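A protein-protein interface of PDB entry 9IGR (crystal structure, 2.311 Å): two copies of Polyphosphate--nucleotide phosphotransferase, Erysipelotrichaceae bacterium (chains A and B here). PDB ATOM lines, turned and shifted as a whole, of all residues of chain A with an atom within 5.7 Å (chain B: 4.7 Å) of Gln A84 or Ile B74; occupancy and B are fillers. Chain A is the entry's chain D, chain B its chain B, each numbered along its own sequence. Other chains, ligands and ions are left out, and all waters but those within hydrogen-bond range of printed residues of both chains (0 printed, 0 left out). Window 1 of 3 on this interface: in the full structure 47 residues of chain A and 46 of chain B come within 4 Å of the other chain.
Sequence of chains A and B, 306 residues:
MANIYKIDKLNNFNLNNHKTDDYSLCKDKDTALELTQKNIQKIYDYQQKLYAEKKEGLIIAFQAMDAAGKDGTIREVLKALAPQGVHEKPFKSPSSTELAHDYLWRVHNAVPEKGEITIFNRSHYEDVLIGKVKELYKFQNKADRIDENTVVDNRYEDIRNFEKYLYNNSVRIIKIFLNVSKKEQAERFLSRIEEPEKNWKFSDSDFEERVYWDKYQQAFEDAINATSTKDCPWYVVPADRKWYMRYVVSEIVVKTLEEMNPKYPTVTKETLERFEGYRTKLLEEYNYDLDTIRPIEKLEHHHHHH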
ATOM      1  N   GLN A  47      30.000  10.227 -21.058  1.00  0.00           N
ATOM      2  CA  GLN A  47      28.775   9.493 -20.860  1.00  0.00           C
ATOM      3  C   GLN A  47      28.823   8.650 -19.608  1.00  0.00           C
ATOM      4  O   GLN A  47      27.848   8.595 -18.909  1.00  0.00           O
ATOM      5  CB  GLN A  47      28.449   8.551 -22.023  1.00  0.00           C
ATOM      6  CG  GLN A  47      27.309   7.564 -21.753  1.00  0.00           C
ATOM      7  CD  GLN A  47      27.374   6.346 -22.653  1.00  0.00           C
ATOM      8  OE1 GLN A  47      28.430   5.784 -22.999  1.00  0.00           O
ATOM      9  NE2 GLN A  47      26.216   5.935 -23.117  1.00  0.00           N
ATOM     10  N   GLN A  48      29.954   8.041 -19.265  1.00  0.00           N
ATOM     11  CA  GLN A  48      30.046   7.230 -18.041  1.00  0.00           C
ATOM     12  C   GLN A  48      29.848   8.091 -16.797  1.00  0.00           C
ATOM     13  O   GLN A  48      29.163   7.685 -15.861  1.00  0.00           O
ATOM     14  CB  GLN A  48      31.365   6.478 -17.901  1.00  0.00           C
ATOM     15  CG  GLN A  48      31.720   5.658 -19.148  1.00  0.00           C
ATOM     16  CD  GLN A  48      30.559   4.765 -19.605  1.00  0.00           C
ATOM     17  OE1 GLN A  48      30.013   3.931 -18.898  1.00  0.00           O
ATOM     18  NE2 GLN A  48      30.089   4.965 -20.811  1.00  0.00           N
ATOM     19  N   TYR A  51      26.023   9.175 -16.657  1.00  0.00           N
ATOM     20  CA  TYR A  51      25.186   8.089 -16.188  1.00  0.00           C
ATOM     21  C   TYR A  51      25.349   7.891 -14.684  1.00  0.00           C
ATOM     22  O   TYR A  51      24.407   7.560 -13.973  1.00  0.00           O
ATOM     23  CB  TYR A  51      25.518   6.774 -16.894  1.00  0.00           C
ATOM     24  CG  TYR A  51      24.556   5.634 -16.637  1.00  0.00           C
ATOM     25  CD1 TYR A  51      23.245   5.669 -17.112  1.00  0.00           C
ATOM     26  CD2 TYR A  51      24.972   4.487 -15.964  1.00  0.00           C
ATOM     27  CE1 TYR A  51      22.360   4.618 -16.864  1.00  0.00           C
ATOM     28  CE2 TYR A  51      24.121   3.409 -15.755  1.00  0.00           C
ATOM     29  CZ  TYR A  51      22.809   3.489 -16.191  1.00  0.00           C
ATOM     30  OH  TYR A  51      22.034   2.396 -15.977  1.00  0.00           O
ATOM     31  N   ALA A  82      28.341   3.467 -24.765  1.00  0.00           N
ATOM     32  CA  ALA A  82      27.965   2.201 -24.170  1.00  0.00           C
ATOM     33  C   ALA A  82      26.455   2.090 -24.256  1.00  0.00           C
ATOM     34  O   ALA A  82      25.832   3.123 -24.321  1.00  0.00           O
ATOM     35  CB  ALA A  82      28.419   2.195 -22.763  1.00  0.00           C
ATOM     36  N   PRO A  83      25.829   0.906 -24.248  1.00  0.00           N
ATOM     37  CA  PRO A  83      24.373   0.806 -24.362  1.00  0.00           C
ATOM     38  C   PRO A  83      23.615   1.381 -23.161  1.00  0.00           C
ATOM     39  O   PRO A  83      22.514   1.807 -23.281  1.00  0.00           O
ATOM     40  CB  PRO A  83      24.096  -0.674 -24.527  1.00  0.00           C
ATOM     41  CG  PRO A  83      25.442  -1.333 -24.666  1.00  0.00           C
ATOM     42  CD  PRO A  83      26.497  -0.384 -24.139  1.00  0.00           C
ATOM     43  N   GLN A  84      24.213   1.456 -21.996  1.00  0.00           N
ATOM     44  CA  GLN A  84      23.510   1.897 -20.801  1.00  0.00           C
ATOM     45  C   GLN A  84      23.085   3.370 -20.909  1.00  0.00           C
ATOM     46  O   GLN A  84      23.832   4.283 -21.171  1.00  0.00           O
ATOM     47  CB  GLN A  84      24.287   1.701 -19.494  1.00  0.00           C
ATOM     48  CG  GLN A  84      24.516   0.233 -19.080  1.00  0.00           C
ATOM     49  CD  GLN A  84      25.826  -0.358 -19.597  1.00  0.00           C
ATOM     50  OE1 GLN A  84      26.451   0.113 -20.571  1.00  0.00           O
ATOM     51  NE2 GLN A  84      26.255  -1.431 -18.963  1.00  0.00           N
ATOM     52  N   GLY A  85      21.817   3.589 -20.610  1.00  0.00           N
ATOM     53  CA  GLY A  85      21.254   4.914 -20.649  1.00  0.00           C
ATOM     54  C   GLY A  85      21.048   5.485 -22.036  1.00  0.00           C
ATOM     55  O   GLY A  85      20.983   6.691 -22.183  1.00  0.00           O
ATOM     56  N   VAL A  86      20.899   4.646 -23.062  1.00  0.00           N
ATOM     57  CA  VAL A  86      20.862   5.163 -24.410  1.00  0.00           C
ATOM     58  C   VAL A  86      19.631   4.629 -25.098  1.00  0.00           C
ATOM     59  O   VAL A  86      19.380   3.470 -24.961  1.00  0.00           O
ATOM     60  CB  VAL A  86      22.116   4.872 -25.247  1.00  0.00           C
ATOM     61  CG1 VAL A  86      21.915   5.327 -26.690  1.00  0.00           C
ATOM     62  CG2 VAL A  86      23.276   5.656 -24.671  1.00  0.00           C
ATOM     63  N   PHE B  62      21.173 -10.848 -18.916  1.00  0.00           N
ATOM     64  CA  PHE B  62      22.215 -11.189 -17.981  1.00  0.00           C
ATOM     65  C   PHE B  62      21.626 -11.262 -16.598  1.00  0.00           C
ATOM     66  O   PHE B  62      21.142 -10.264 -16.108  1.00  0.00           O
ATOM     67  CB  PHE B  62      23.260 -10.084 -17.975  1.00  0.00           C
ATOM     68  CG  PHE B  62      24.068  -9.978 -19.257  1.00  0.00           C
ATOM     69  CD1 PHE B  62      23.668  -9.159 -20.279  1.00  0.00           C
ATOM     70  CD2 PHE B  62      25.254 -10.656 -19.402  1.00  0.00           C
ATOM     71  CE1 PHE B  62      24.390  -9.083 -21.462  1.00  0.00           C
ATOM     72  CE2 PHE B  62      25.977 -10.582 -20.575  1.00  0.00           C
ATOM     73  CZ  PHE B  62      25.555  -9.798 -21.597  1.00  0.00           C
ATOM     74  N   LYS B  70      27.937  -7.938 -14.795  1.00  0.00           N
ATOM     75  CA  LYS B  70      26.903  -7.668 -15.778  1.00  0.00           C
ATOM     76  C   LYS B  70      27.109  -6.345 -16.527  1.00  0.00           C
ATOM     77  O   LYS B  70      27.213  -6.353 -17.745  1.00  0.00           O
ATOM     78  CB  LYS B  70      25.522  -7.698 -15.149  1.00  0.00           C
ATOM     79  CG  LYS B  70      25.069  -9.029 -14.530  1.00  0.00           C
ATOM     80  CD  LYS B  70      23.773  -8.984 -13.684  1.00  0.00           C
ATOM     81  CE  LYS B  70      23.660  -7.823 -12.652  1.00  0.00           C
ATOM     82  NZ  LYS B  70      24.487  -8.103 -11.472  1.00  0.00           N
ATOM     83  N   ASP B  71      27.194  -5.216 -15.813  1.00  0.00           N
ATOM     84  CA  ASP B  71      27.375  -3.927 -16.440  1.00  0.00           C
ATOM     85  C   ASP B  71      28.687  -3.836 -17.202  1.00  0.00           C
ATOM     86  O   ASP B  71      28.743  -3.221 -18.230  1.00  0.00           O
ATOM     87  CB  ASP B  71      27.145  -2.756 -15.488  1.00  0.00           C
ATOM     88  CG  ASP B  71      25.686  -2.252 -15.367  1.00  0.00           C
ATOM     89  OD1 ASP B  71      24.873  -2.262 -16.411  1.00  0.00           O
ATOM     90  OD2 ASP B  71      25.309  -1.845 -14.239  1.00  0.00           O
ATOM     91  N   GLY B  72      29.785  -4.340 -16.692  1.00  0.00           N
ATOM     92  CA  GLY B  72      31.054  -4.153 -17.385  1.00  0.00           C
ATOM     93  C   GLY B  72      31.127  -5.094 -18.580  1.00  0.00           C
ATOM     94  O   GLY B  72      31.746  -4.752 -19.581  1.00  0.00           O
ATOM     95  N   THR B  73      30.451  -6.244 -18.534  1.00  0.00           N
ATOM     96  CA  THR B  73      30.432  -7.085 -19.720  1.00  0.00           C
ATOM     97  C   THR B  73      29.539  -6.463 -20.798  1.00  0.00           C
ATOM     98  O   THR B  73      29.906  -6.399 -21.974  1.00  0.00           O
ATOM     99  CB  THR B  73      29.995  -8.495 -19.352  1.00  0.00           C
ATOM    100  OG1 THR B  73      30.960  -8.955 -18.409  1.00  0.00           O
ATOM    101  CG2 THR B  73      29.937  -9.382 -20.577  1.00  0.00           C
ATOM    102  N   ILE B  74      28.333  -6.027 -20.436  1.00  0.00           N
ATOM    103  CA  ILE B  74      27.448  -5.334 -21.377  1.00  0.00           C
ATOM    104  C   ILE B  74      28.199  -4.137 -22.008  1.00  0.00           C
ATOM    105  O   ILE B  74      28.143  -3.919 -23.189  1.00  0.00           O
ATOM    106  CB  ILE B  74      26.212  -4.843 -20.606  1.00  0.00           C
ATOM    107  CG1 ILE B  74      25.305  -5.994 -20.277  1.00  0.00           C
ATOM    108  CG2 ILE B  74      25.508  -3.643 -21.250  1.00  0.00           C
ATOM    109  CD1 ILE B  74      24.257  -5.647 -19.237  1.00  0.00           C
ATOM    110  N   ARG B  75      28.905  -3.346 -21.221  1.00  0.00           N
ATOM    111  CA  ARG B  75      29.666  -2.217 -21.686  1.00  0.00           C
ATOM    112  C   ARG B  75      30.817  -2.629 -22.597  1.00  0.00           C
ATOM    113  O   ARG B  75      30.959  -2.092 -23.703  1.00  0.00           O
ATOM    114  CB  ARG B  75      30.190  -1.373 -20.522  1.00  0.00           C
ATOM    115  CG  ARG B  75      31.098  -0.270 -21.025  1.00  0.00           C
ATOM    116  CD  ARG B  75      30.993   0.969 -20.145  1.00  0.00           C
ATOM    117  NE  ARG B  75      31.814   0.718 -18.969  1.00  0.00           N
ATOM    118  CZ  ARG B  75      31.398   0.590 -17.733  1.00  0.00           C
ATOM    119  NH1 ARG B  75      30.161   0.106 -17.492  1.00  0.00           N
ATOM    120  NH2 ARG B  75      32.282   0.798 -16.768  1.00  0.00           N
ATOM    121  N   GLU B  76      31.656  -3.573 -22.195  1.00  0.00           N
ATOM    122  CA  GLU B  76      32.836  -3.832 -23.009  1.00  0.00           C
ATOM    123  C   GLU B  76      32.520  -4.611 -24.287  1.00  0.00           C
ATOM    124  O   GLU B  76      33.084  -4.296 -25.330  1.00  0.00           O
ATOM    125  CB  GLU B  76      33.930  -4.399 -22.104  1.00  0.00           C
ATOM    126  CG  GLU B  76      35.176  -3.514 -22.199  1.00  0.00           C
ATOM    127  CD  GLU B  76      35.982  -3.860 -23.427  1.00  0.00           C
ATOM    128  OE1 GLU B  76      35.706  -4.982 -23.985  1.00  0.00           O
ATOM    129  OE2 GLU B  76      36.879  -3.010 -23.754  1.00  0.00           O
ATOM    130  N   VAL B  77      31.549  -5.522 -24.263  1.00  0.00           N
ATOM    131  CA  VAL B  77      31.268  -6.340 -25.443  1.00  0.00           C
ATOM    132  C   VAL B  77      30.235  -5.675 -26.353  1.00  0.00           C
ATOM    133  O   VAL B  77      30.407  -5.675 -27.551  1.00  0.00           O
ATOM    134  CB  VAL B  77      30.762  -7.723 -25.010  1.00  0.00           C
ATOM    135  CG1 VAL B  77      30.342  -8.583 -26.182  1.00  0.00           C
ATOM    136  CG2 VAL B  77      31.782  -8.454 -24.172  1.00  0.00           C
ATOM    137  N   LEU B  78      29.183  -5.078 -25.809  1.00  0.00           N
ATOM    138  CA  LEU B  78      28.104  -4.577 -26.646  1.00  0.00           C
ATOM    139  C   LEU B  78      28.186  -3.079 -26.945  1.00  0.00           C
ATOM    140  O   LEU B  78      27.314  -2.582 -27.615  1.00  0.00           O
ATOM    141  CB  LEU B  78      26.768  -4.958 -26.002  1.00  0.00           C
ATOM    142  CG  LEU B  78      26.580  -6.472 -25.891  1.00  0.00           C
ATOM    143  CD1 LEU B  78      25.349  -6.789 -25.149  1.00  0.00           C
ATOM    144  CD2 LEU B  78      26.571  -7.260 -27.245  1.00  0.00           C
ATOM    145  N   LYS B  79      29.180  -2.350 -26.493  1.00  0.00           N
ATOM    146  CA  LYS B  79      29.361  -0.976 -26.926  1.00  0.00           C
ATOM    147  C   LYS B  79      29.765  -0.926 -28.410  1.00  0.00           C
ATOM    148  O   LYS B  79      29.732   0.131 -29.009  1.00  0.00           O
ATOM    149  CB  LYS B  79      30.425  -0.155 -26.179  1.00  0.00           C
ATOM    150  CG  LYS B  79      31.848  -0.677 -26.368  1.00  0.00           C
ATOM    151  CD  LYS B  79      32.913   0.129 -25.619  1.00  0.00           C
ATOM    152  CE  LYS B  79      34.246  -0.390 -26.080  1.00  0.00           C
ATOM    153  NZ  LYS B  79      35.320  -0.098 -25.130  1.00  0.00           N
ATOM    154  N   GLU B  88      18.656  -0.832 -23.514  1.00  0.00           N
ATOM    155  CA  GLU B  88      19.197  -1.561 -22.357  1.00  0.00           C
ATOM    156  C   GLU B  88      18.156  -1.316 -21.260  1.00  0.00           C
ATOM    157  O   GLU B  88      17.652  -0.219 -21.064  1.00  0.00           O
ATOM    158  CB  GLU B  88      20.636  -1.220 -21.927  1.00  0.00           C
ATOM    159  CG  GLU B  88      21.195  -1.993 -20.711  1.00  0.00           C
ATOM    160  CD  GLU B  88      21.133  -1.408 -19.258  1.00  0.00           C
ATOM    161  OE1 GLU B  88      20.558  -0.315 -19.197  1.00  0.00           O
ATOM    162  OE2 GLU B  88      21.640  -1.870 -18.173  1.00  0.00           O
ATOM    163  N   ILE B 119      18.789  -5.347 -24.333  1.00  0.00           N
ATOM    164  CA  ILE B 119      19.655  -5.957 -23.351  1.00  0.00           C
ATOM    165  C   ILE B 119      18.964  -5.864 -22.022  1.00  0.00           C
ATOM    166  O   ILE B 119      18.587  -4.781 -21.614  1.00  0.00           O
ATOM    167  CB  ILE B 119      21.007  -5.230 -23.337  1.00  0.00           C
ATOM    168  CG1 ILE B 119      21.682  -5.346 -24.672  1.00  0.00           C
ATOM    169  CG2 ILE B 119      21.907  -5.737 -22.242  1.00  0.00           C
ATOM    170  CD1 ILE B 119      22.713  -4.243 -24.880  1.00  0.00           C
ATOM    171  N   ASN B 121      19.464  -6.239 -18.070  1.00  0.00           N
ATOM    172  CA  ASN B 121      20.277  -6.361 -16.901  1.00  0.00           C
ATOM    173  C   ASN B 121      19.397  -6.795 -15.748  1.00  0.00           C
ATOM    174  O   ASN B 121      18.665  -5.998 -15.194  1.00  0.00           O
ATOM    175  CB  ASN B 121      21.017  -5.067 -16.670  1.00  0.00           C
ATOM    176  CG  ASN B 121      21.939  -5.183 -15.479  1.00  0.00           C
ATOM    177  OD1 ASN B 121      21.758  -6.033 -14.605  1.00  0.00           O
ATOM    178  ND2 ASN B 121      22.860  -4.250 -15.376  1.00  0.00           N
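The side-chain amide nitrogen (NE2) of Gln A84 is in hydrogen-bond range of the side-chain carboxylate (OD1) of Asp B71, at 3.0 Å.
The side-chain carboxylate (OD1) of Asp B71 sits at hydrogen-bond distance from the side-chain amide nitrogen (ND2) of Asn B121 (3.0 Å).
The side-chain carboxylate (OE2) of Glu B76 is in salt-bridge range of the side-chain amino group (NZ) of Lys B79.
The side-chain amide oxygen (OE1) of Gln A47 is in hydrogen-bond range of the side-chain amide nitrogen (NE2) of Gln A48, at 2.9 Å.
The side-chain amide oxygen (OE1) of Gln A47 is in hydrogen-bond range of the backbone NH (N) of Ala A82, 2.9 Å away.
The side-chain amide nitrogen (NE2) of Gln A47 is in hydrogen-bond range of the backbone carbonyl oxygen (O) of Gln A84 (3.5 Å).
Among the printed residues, pairs that only touch across the chains: Gln A48 with Arg B75, Ala A82 with Arg B75, Ala A82 with Lys B79, Pro A83 with Leu B78, Pro A83 with Glu B88, Pro A83 with Ile B119, Gln A84 with Ile B74, Gln A84 with Arg B75 and Gln A84 with Glu B88.
Of chain B, only Asp B71, Ile B74, Arg B75 and Glu B88 come within 4 Å of Gln A84.
Of the printed residues of chain A, Ile B74 touches Gln A84 (3.3 Å).
Printed residues of chain B within 4 Å of Gln A48: Arg B75 (3.4 Å).
Printed residues of chain B within 4 Å of Pro A83: Leu B78 (3.7 Å), Glu B88 (3.8 Å) and Ile B119 (3.8 Å).
Of the printed residues of chain A, Lys B79 touches Ala A82.
Printed residues of chain A within 4 Å of Leu B78: Pro A83 (3.7 Å).
Of the printed residues of chain A, Arg B75 touches Gln A48, Ala A82 and Gln A84.
The nearest printed residue of chain B that does not touch Gln A84 is Gly B72 (5.1 Å).
The nearest printed residue of chain B that does not touch Gln A48 is Asp B71 (7.3 Å).
Of the 14 printed residues of chain B, 7 touch a printed residue of chain A.
Hydrophobic or aromatic side chains of chain B that line the printed part of chain A: Ile B74 and Ile B119.
Hydrophobic or aromatic side chains of chain A that line the printed part of chain B: Ala A82 and Pro A83.
Among the printed residues, 10 pairs touch across the chains.
Among the printed residues, no Asp or Glu carboxylate lies within 4 Å of a Lys or Arg side-chain nitrogen of the other chain.
No position is printed for both chains.
Of the 10 pairs that touch across the chains among the printed residues, none has its exchanged pair printed and touching as well.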
